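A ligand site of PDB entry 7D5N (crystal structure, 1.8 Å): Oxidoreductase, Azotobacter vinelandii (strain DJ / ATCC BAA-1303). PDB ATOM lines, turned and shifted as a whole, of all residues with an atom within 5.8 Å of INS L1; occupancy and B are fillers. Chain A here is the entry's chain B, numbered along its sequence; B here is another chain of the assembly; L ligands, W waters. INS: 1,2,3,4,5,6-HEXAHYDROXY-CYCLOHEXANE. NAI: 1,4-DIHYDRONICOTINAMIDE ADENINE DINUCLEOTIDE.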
ATOM      1  N   GLN A  24     -22.026  27.731   1.711  1.00  0.00           N
ATOM      2  CA  GLN A  24     -22.778  27.950   2.973  1.00  0.00           C
ATOM      3  C   GLN A  24     -21.822  28.402   4.078  1.00  0.00           C
ATOM      4  O   GLN A  24     -22.208  29.298   4.837  1.00  0.00           O
ATOM      5  CB  GLN A  24     -23.526  26.703   3.385  1.00  0.00           C
ATOM      6  CG  GLN A  24     -24.598  26.289   2.391  1.00  0.00           C
ATOM      7  CD  GLN A  24     -25.408  25.106   2.875  1.00  0.00           C
ATOM      8  OE1 GLN A  24     -24.882  24.198   3.536  1.00  0.00           O
ATOM      9  NE2 GLN A  24     -26.683  25.112   2.540  1.00  0.00           N
ATOM     10  N   ILE A  25     -20.645  27.811   4.165  1.00  0.00           N
ATOM     11  CA  ILE A  25     -19.815  27.954   5.405  1.00  0.00           C
ATOM     12  C   ILE A  25     -18.568  28.811   5.156  1.00  0.00           C
ATOM     13  O   ILE A  25     -17.910  29.163   6.147  1.00  0.00           O
ATOM     14  CB  ILE A  25     -19.488  26.559   5.993  1.00  0.00           C
ATOM     15  CG1 ILE A  25     -19.420  26.620   7.526  1.00  0.00           C
ATOM     16  CG2 ILE A  25     -18.225  25.989   5.393  1.00  0.00           C
ATOM     17  CD1 ILE A  25     -20.723  27.058   8.176  1.00  0.00           C
ATOM     18  N   LYS A 115     -15.360  19.576   9.498  1.00  0.00           N
ATOM     19  CA  LYS A 115     -15.991  18.294   9.889  1.00  0.00           C
ATOM     20  C   LYS A 115     -16.883  17.824   8.747  1.00  0.00           C
ATOM     21  O   LYS A 115     -17.402  18.650   7.998  1.00  0.00           O
ATOM     22  CB  LYS A 115     -16.809  18.503  11.175  1.00  0.00           C
ATOM     23  CG  LYS A 115     -17.771  19.684  11.088  1.00  0.00           C
ATOM     24  CD  LYS A 115     -19.187  19.331  11.398  1.00  0.00           C
ATOM     25  CE  LYS A 115     -19.779  18.251  10.519  1.00  0.00           C
ATOM     26  NZ  LYS A 115     -20.583  18.832   9.424  1.00  0.00           N
ATOM     27  N   TYR A 144     -19.632  24.971  17.505  1.00  0.00           N
ATOM     28  CA  TYR A 144     -20.544  25.185  18.650  1.00  0.00           C
ATOM     29  C   TYR A 144     -19.754  25.066  19.957  1.00  0.00           C
ATOM     30  O   TYR A 144     -20.186  25.642  20.978  1.00  0.00           O
ATOM     31  CB  TYR A 144     -21.728  24.215  18.561  1.00  0.00           C
ATOM     32  CG  TYR A 144     -22.491  24.335  17.273  1.00  0.00           C
ATOM     33  CD1 TYR A 144     -23.420  25.342  17.057  1.00  0.00           C
ATOM     34  CD2 TYR A 144     -22.259  23.430  16.244  1.00  0.00           C
ATOM     35  CE1 TYR A 144     -24.101  25.461  15.861  1.00  0.00           C
ATOM     36  CE2 TYR A 144     -22.914  23.548  15.022  1.00  0.00           C
ATOM     37  CZ  TYR A 144     -23.842  24.565  14.840  1.00  0.00           C
ATOM     38  OH  TYR A 144     -24.504  24.663  13.656  1.00  0.00           O
ATOM     39  N   PHE A 172     -29.296  16.682  16.936  1.00  0.00           N
ATOM     40  CA  PHE A 172     -29.240  17.771  15.950  1.00  0.00           C
ATOM     41  C   PHE A 172     -30.230  17.368  14.888  1.00  0.00           C
ATOM     42  O   PHE A 172     -29.939  16.512  14.058  1.00  0.00           O
ATOM     43  CB  PHE A 172     -27.808  17.953  15.452  1.00  0.00           C
ATOM     44  CG  PHE A 172     -27.532  19.244  14.742  1.00  0.00           C
ATOM     45  CD1 PHE A 172     -26.247  19.751  14.719  1.00  0.00           C
ATOM     46  CD2 PHE A 172     -28.542  19.978  14.124  1.00  0.00           C
ATOM     47  CE1 PHE A 172     -25.965  20.930  14.058  1.00  0.00           C
ATOM     48  CE2 PHE A 172     -28.266  21.182  13.491  1.00  0.00           C
ATOM     49  CZ  PHE A 172     -26.965  21.649  13.456  1.00  0.00           C
ATOM     50  N   HIS A 174     -32.920  18.985  12.382  1.00  0.00           N
ATOM     51  CA  HIS A 174     -33.530  20.121  11.641  1.00  0.00           C
ATOM     52  C   HIS A 174     -34.466  19.554  10.565  1.00  0.00           C
ATOM     53  O   HIS A 174     -34.414  18.326  10.329  1.00  0.00           O
ATOM     54  CB  HIS A 174     -32.466  21.063  11.085  1.00  0.00           C
ATOM     55  CG  HIS A 174     -31.622  20.469  10.006  1.00  0.00           C
ATOM     56  ND1 HIS A 174     -32.080  20.376   8.688  1.00  0.00           N
ATOM     57  CD2 HIS A 174     -30.381  19.941  10.038  1.00  0.00           C
ATOM     58  CE1 HIS A 174     -31.130  19.812   7.964  1.00  0.00           C
ATOM     59  NE2 HIS A 174     -30.082  19.535   8.767  1.00  0.00           N
ATOM     60  N   PHE A 176     -34.791  21.045   7.292  1.00  0.00           N
ATOM     61  CA  PHE A 176     -34.529  21.692   5.977  1.00  0.00           C
ATOM     62  C   PHE A 176     -34.583  20.689   4.826  1.00  0.00           C
ATOM     63  O   PHE A 176     -34.909  21.133   3.712  1.00  0.00           O
ATOM     64  CB  PHE A 176     -33.233  22.512   5.985  1.00  0.00           C
ATOM     65  CG  PHE A 176     -33.335  23.762   6.809  1.00  0.00           C
ATOM     66  CD1 PHE A 176     -34.076  24.858   6.368  1.00  0.00           C
ATOM     67  CD2 PHE A 176     -32.660  23.872   8.008  1.00  0.00           C
ATOM     68  CE1 PHE A 176     -34.155  26.002   7.141  1.00  0.00           C
ATOM     69  CE2 PHE A 176     -32.732  25.018   8.766  1.00  0.00           C
ATOM     70  CZ  PHE A 176     -33.477  26.084   8.336  1.00  0.00           C
ATOM     71  N   HIS A 177     -34.354  19.399   5.073  1.00  0.00           N
ATOM     72  CA  HIS A 177     -34.368  18.410   3.970  1.00  0.00           C
ATOM     73  C   HIS A 177     -35.541  17.440   4.093  1.00  0.00           C
ATOM     74  O   HIS A 177     -35.456  16.353   3.514  1.00  0.00           O
ATOM     75  CB  HIS A 177     -32.996  17.746   3.808  1.00  0.00           C
ATOM     76  CG  HIS A 177     -31.906  18.742   3.630  1.00  0.00           C
ATOM     77  ND1 HIS A 177     -30.636  18.531   4.129  1.00  0.00           N
ATOM     78  CD2 HIS A 177     -31.892  19.956   3.027  1.00  0.00           C
ATOM     79  CE1 HIS A 177     -29.885  19.584   3.855  1.00  0.00           C
ATOM     80  NE2 HIS A 177     -30.627  20.464   3.164  1.00  0.00           N
ATOM     81  N   ARG A 191     -24.223  16.272  -0.385  1.00  0.00           N
ATOM     82  CA  ARG A 191     -24.459  15.606   0.927  1.00  0.00           C
ATOM     83  C   ARG A 191     -25.178  14.271   0.735  1.00  0.00           C
ATOM     84  O   ARG A 191     -24.965  13.416   1.572  1.00  0.00           O
ATOM     85  CB  ARG A 191     -25.226  16.539   1.865  1.00  0.00           C
ATOM     86  CG  ARG A 191     -24.314  17.559   2.518  1.00  0.00           C
ATOM     87  CD  ARG A 191     -25.102  18.591   3.255  1.00  0.00           C
ATOM     88  NE  ARG A 191     -24.270  19.407   4.114  1.00  0.00           N
ATOM     89  CZ  ARG A 191     -23.640  20.516   3.726  1.00  0.00           C
ATOM     90  NH1 ARG A 191     -23.713  20.933   2.471  1.00  0.00           N
ATOM     91  NH2 ARG A 191     -22.907  21.191   4.599  1.00  0.00           N
ATOM     92  N   TYR A 201     -24.962  10.398   5.694  1.00  0.00           N
ATOM     93  CA  TYR A 201     -25.365  11.819   5.573  1.00  0.00           C
ATOM     94  C   TYR A 201     -25.484  12.423   6.983  1.00  0.00           C
ATOM     95  O   TYR A 201     -24.478  12.942   7.469  1.00  0.00           O
ATOM     96  CB  TYR A 201     -26.539  11.978   4.606  1.00  0.00           C
ATOM     97  CG  TYR A 201     -27.197  13.330   4.713  1.00  0.00           C
ATOM     98  CD1 TYR A 201     -26.439  14.450   5.011  1.00  0.00           C
ATOM     99  CD2 TYR A 201     -28.564  13.498   4.574  1.00  0.00           C
ATOM    100  CE1 TYR A 201     -27.010  15.700   5.169  1.00  0.00           C
ATOM    101  CE2 TYR A 201     -29.155  14.740   4.709  1.00  0.00           C
ATOM    102  CZ  TYR A 201     -28.370  15.839   5.035  1.00  0.00           C
ATOM    103  OH  TYR A 201     -28.878  17.087   5.204  1.00  0.00           O
ATOM    104  N   ASP A 205     -22.950  14.662   9.221  1.00  0.00           N
ATOM    105  CA  ASP A 205     -23.215  16.080   8.874  1.00  0.00           C
ATOM    106  C   ASP A 205     -23.652  16.836  10.136  1.00  0.00           C
ATOM    107  O   ASP A 205     -23.198  17.971  10.316  1.00  0.00           O
ATOM    108  CB  ASP A 205     -24.288  16.185   7.792  1.00  0.00           C
ATOM    109  CG  ASP A 205     -24.399  17.576   7.210  1.00  0.00           C
ATOM    110  OD1 ASP A 205     -23.390  18.073   6.664  1.00  0.00           O
ATOM    111  OD2 ASP A 205     -25.490  18.167   7.339  1.00  0.00           O
ATOM    112  N   VAL A 206     -24.535  16.258  10.963  1.00  0.00           N
ATOM    113  CA  VAL A 206     -25.088  16.989  12.139  1.00  0.00           C
ATOM    114  C   VAL A 206     -24.895  16.186  13.447  1.00  0.00           C
ATOM    115  O   VAL A 206     -24.709  16.816  14.483  1.00  0.00           O
ATOM    116  CB  VAL A 206     -26.549  17.427  11.916  1.00  0.00           C
ATOM    117  CG1 VAL A 206     -26.641  18.490  10.816  1.00  0.00           C
ATOM    118  CG2 VAL A 206     -27.498  16.277  11.632  1.00  0.00           C
ATOM    119  N   HIS A 209     -21.831  16.936  15.779  1.00  0.00           N
ATOM    120  CA  HIS A 209     -21.751  18.233  16.505  1.00  0.00           C
ATOM    121  C   HIS A 209     -22.038  18.043  17.994  1.00  0.00           C
ATOM    122  O   HIS A 209     -21.183  18.363  18.828  1.00  0.00           O
ATOM    123  CB  HIS A 209     -22.605  19.300  15.816  1.00  0.00           C
ATOM    124  CG  HIS A 209     -21.938  19.935  14.642  1.00  0.00           C
ATOM    125  ND1 HIS A 209     -20.751  20.642  14.774  1.00  0.00           N
ATOM    126  CD2 HIS A 209     -22.302  20.036  13.350  1.00  0.00           C
ATOM    127  CE1 HIS A 209     -20.409  21.133  13.601  1.00  0.00           C
ATOM    128  NE2 HIS A 209     -21.334  20.776  12.701  1.00  0.00           N
ATOM    129  N   HIS A 269     -33.274  24.121  13.611  1.00  0.00           N
ATOM    130  CA  HIS A 269     -31.885  23.665  13.861  1.00  0.00           C
ATOM    131  C   HIS A 269     -31.934  22.522  14.886  1.00  0.00           C
ATOM    132  O   HIS A 269     -31.567  21.393  14.527  1.00  0.00           O
ATOM    133  CB  HIS A 269     -30.989  24.824  14.335  1.00  0.00           C
ATOM    134  CG  HIS A 269     -29.769  24.962  13.495  1.00  0.00           C
ATOM    135  ND1 HIS A 269     -28.486  24.992  14.033  1.00  0.00           N
ATOM    136  CD2 HIS A 269     -29.624  25.070  12.150  1.00  0.00           C
ATOM    137  CE1 HIS A 269     -27.613  25.142  13.054  1.00  0.00           C
ATOM    138  NE2 HIS A 269     -28.282  25.165  11.892  1.00  0.00           N
ATOM    139  N   HIS B 325     -28.808  29.067  12.323  1.00  0.00           N
ATOM    140  CA  HIS B 325     -27.535  29.423  13.008  1.00  0.00           C
ATOM    141  C   HIS B 325     -27.733  30.773  13.673  1.00  0.00           C
ATOM    142  O   HIS B 325     -28.077  31.721  12.971  1.00  0.00           O
ATOM    143  CB  HIS B 325     -26.349  29.521  12.047  1.00  0.00           C
ATOM    144  CG  HIS B 325     -26.085  28.299  11.260  1.00  0.00           C
ATOM    145  ND1 HIS B 325     -26.705  28.061  10.047  1.00  0.00           N
ATOM    146  CD2 HIS B 325     -25.294  27.231  11.503  1.00  0.00           C
ATOM    147  CE1 HIS B 325     -26.281  26.909   9.575  1.00  0.00           C
ATOM    148  NE2 HIS B 325     -25.432  26.387  10.442  1.00  0.00           N
HETATM  149  C1  INS L   1     -25.938  22.146   8.908  1.00  0.00           C
HETATM  150  C2  INS L   1     -25.342  22.995  10.002  1.00  0.00           C
HETATM  151  C3  INS L   1     -24.220  22.256  10.719  1.00  0.00           C
HETATM  152  C4  INS L   1     -23.179  21.754   9.719  1.00  0.00           C
HETATM  153  C5  INS L   1     -23.793  21.005   8.547  1.00  0.00           C
HETATM  154  C6  INS L   1     -24.861  21.837   7.885  1.00  0.00           C
HETATM  155  O1  INS L   1     -27.043  22.843   8.328  1.00  0.00           O
HETATM  156  O2  INS L   1     -24.797  24.187   9.425  1.00  0.00           O
HETATM  157  O3  INS L   1     -23.607  23.159  11.669  1.00  0.00           O
HETATM  158  O4  INS L   1     -22.220  20.902  10.325  1.00  0.00           O
HETATM  159  O5  INS L   1     -22.782  20.705   7.573  1.00  0.00           O
HETATM  160  O6  INS L   1     -25.364  21.091   6.801  1.00  0.00           O
HETATM  161  PA  NAI L   2     -21.078  24.125  -0.255  1.00  0.00           P
HETATM  162  O1A NAI L   2     -21.506  23.151  -1.276  1.00  0.00           O
HETATM  163  O2A NAI L   2     -21.989  25.177   0.174  1.00  0.00           O
HETATM  164  O5B NAI L   2     -19.706  24.836  -0.740  1.00  0.00           O
HETATM  165  C5B NAI L   2     -18.596  24.110  -1.251  1.00  0.00           C
HETATM  166  C4B NAI L   2     -17.578  25.155  -1.696  1.00  0.00           C
HETATM  167  O4B NAI L   2     -16.318  24.578  -1.975  1.00  0.00           O
HETATM  168  C3B NAI L   2     -18.000  25.871  -2.973  1.00  0.00           C
HETATM  169  O3B NAI L   2     -17.511  27.216  -2.917  1.00  0.00           O
HETATM  170  C2B NAI L   2     -17.307  25.111  -4.068  1.00  0.00           C
HETATM  171  O2B NAI L   2     -17.069  25.883  -5.238  1.00  0.00           O
HETATM  172  C1B NAI L   2     -16.011  24.843  -3.345  1.00  0.00           C
HETATM  173  N9A NAI L   2     -15.313  23.654  -3.788  1.00  0.00           N
HETATM  174  C8A NAI L   2     -15.804  22.436  -4.031  1.00  0.00           C
HETATM  175  N7A NAI L   2     -14.785  21.610  -4.383  1.00  0.00           N
HETATM  176  C5A NAI L   2     -13.665  22.332  -4.385  1.00  0.00           C
HETATM  177  C6A NAI L   2     -12.262  22.071  -4.659  1.00  0.00           C
HETATM  178  N6A NAI L   2     -11.869  20.852  -5.015  1.00  0.00           N
HETATM  179  N1A NAI L   2     -11.391  23.095  -4.544  1.00  0.00           N
HETATM  180  C2A NAI L   2     -11.796  24.323  -4.147  1.00  0.00           C
HETATM  181  N3A NAI L   2     -13.096  24.633  -3.893  1.00  0.00           N
HETATM  182  C4A NAI L   2     -14.019  23.679  -3.977  1.00  0.00           C
HETATM  183  O3  NAI L   2     -20.626  23.258   0.999  1.00  0.00           O
HETATM  184  PN  NAI L   2     -20.739  23.802   2.505  1.00  0.00           P
HETATM  185  O1N NAI L   2     -22.131  23.590   2.991  1.00  0.00           O
HETATM  186  O2N NAI L   2     -20.117  25.124   2.647  1.00  0.00           O
HETATM  187  O5D NAI L   2     -19.821  22.736   3.251  1.00  0.00           O
HETATM  188  C5D NAI L   2     -18.414  22.698   3.099  1.00  0.00           C
HETATM  189  C4D NAI L   2     -17.769  21.858   4.178  1.00  0.00           C
HETATM  190  O4D NAI L   2     -18.039  22.503   5.445  1.00  0.00           O
HETATM  191  C3D NAI L   2     -18.332  20.464   4.286  1.00  0.00           C
HETATM  192  O3D NAI L   2     -17.321  19.610   4.762  1.00  0.00           O
HETATM  193  C2D NAI L   2     -19.358  20.527   5.383  1.00  0.00           C
HETATM  194  O2D NAI L   2     -19.453  19.335   6.158  1.00  0.00           O
HETATM  195  C1D NAI L   2     -18.773  21.605   6.277  1.00  0.00           C
HETATM  196  N1N NAI L   2     -19.735  22.355   7.052  1.00  0.00           N
HETATM  197  C2N NAI L   2     -19.464  22.529   8.351  1.00  0.00           C
HETATM  198  C3N NAI L   2     -20.301  23.237   9.180  1.00  0.00           C
HETATM  199  C7N NAI L   2     -19.954  23.426  10.609  1.00  0.00           C
HETATM  200  O7N NAI L   2     -20.811  23.840  11.366  1.00  0.00           O
HETATM  201  N7N NAI L   2     -18.692  23.229  10.977  1.00  0.00           N
HETATM  202  C4N NAI L   2     -21.544  23.905   8.653  1.00  0.00           C
HETATM  203  C5N NAI L   2     -21.712  23.672   7.224  1.00  0.00           C
HETATM  204  C6N NAI L   2     -20.807  22.925   6.494  1.00  0.00           C
HETATM  205  O   HOH W   1     -28.570  24.635   9.133  1.00  0.00           O
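NE2 of His 325 of chain B lies within hydrogen-bond range of O2 of INS L1, at 2.5 Å. O4 of INS L1 is in hydrogen-bond range of NE2 of His 209, at 2.5 Å. OH of Tyr 144 is in hydrogen-bond range of O3 of INS L1. The side-chain amino group (NZ) of Lys 115 lies within hydrogen-bond range of an oxygen (O4) of INS L1, 2.8 Å away. O4 of INS L1 is in hydrogen-bond range of O of Asp 205. The side-chain carboxylate (OD1) of Asp 205 sits at hydrogen-bond distance from an oxygen (O5) of INS L1 (2.9 Å). NH2 of Arg 191 is in hydrogen-bond range of O5 of INS L1 (3.0 Å). NE2 of His 209 is in hydrogen-bond range of O7N of NAI L2 (3.4 Å). O of Lys 115 is in hydrogen-bond range of O2D of NAI L2 (2.8 Å). An oxygen (O2D) of NAI L2 is in hydrogen-bond range of the side-chain amino group of Lys 115 (3.5 Å). The guanidinium group of Arg 191 is in salt-bridge range of an oxygen (O1N) of NAI L2, 3.0 Å away. The backbone NH (N) of Gln 24 is in hydrogen-bond range of an oxygen (O2A) of NAI L2. OE1 of Gln 24 sits close to O1N of NAI L2 (2.9 Å). O2N of NAI L2 is in hydrogen-bond range of N of Ile 25 (3.1 Å).
O3 of INS L1 is in hydrogen-bond range of O7N of NAI L2.
A ring nitrogen (NE2) of His 325 of chain B is in hydrogen-bond range of a ring nitrogen (NE2) of His 269 (3.4 Å). NZ of Lys 115 lies within hydrogen-bond range of O of Asp 205, 2.9 Å away. The side-chain carboxylate (OD1) of Asp 205 lies within salt-bridge range of the guanidinium group (NE) of Arg 191 (3.0 Å).
Phe 172 touches INS L1 (CZ to C3, 3.9 Å). Hydrophobic or aromatic side chains within 4 Å of INS L1: Tyr 144, Phe 172, His 209 and His 325 of chain B. The nearest printed residue that does not touch INS L1 is His 269 (4.1 Å).
Water W1 bridges O1 of INS L1 and NE2 of His 269.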
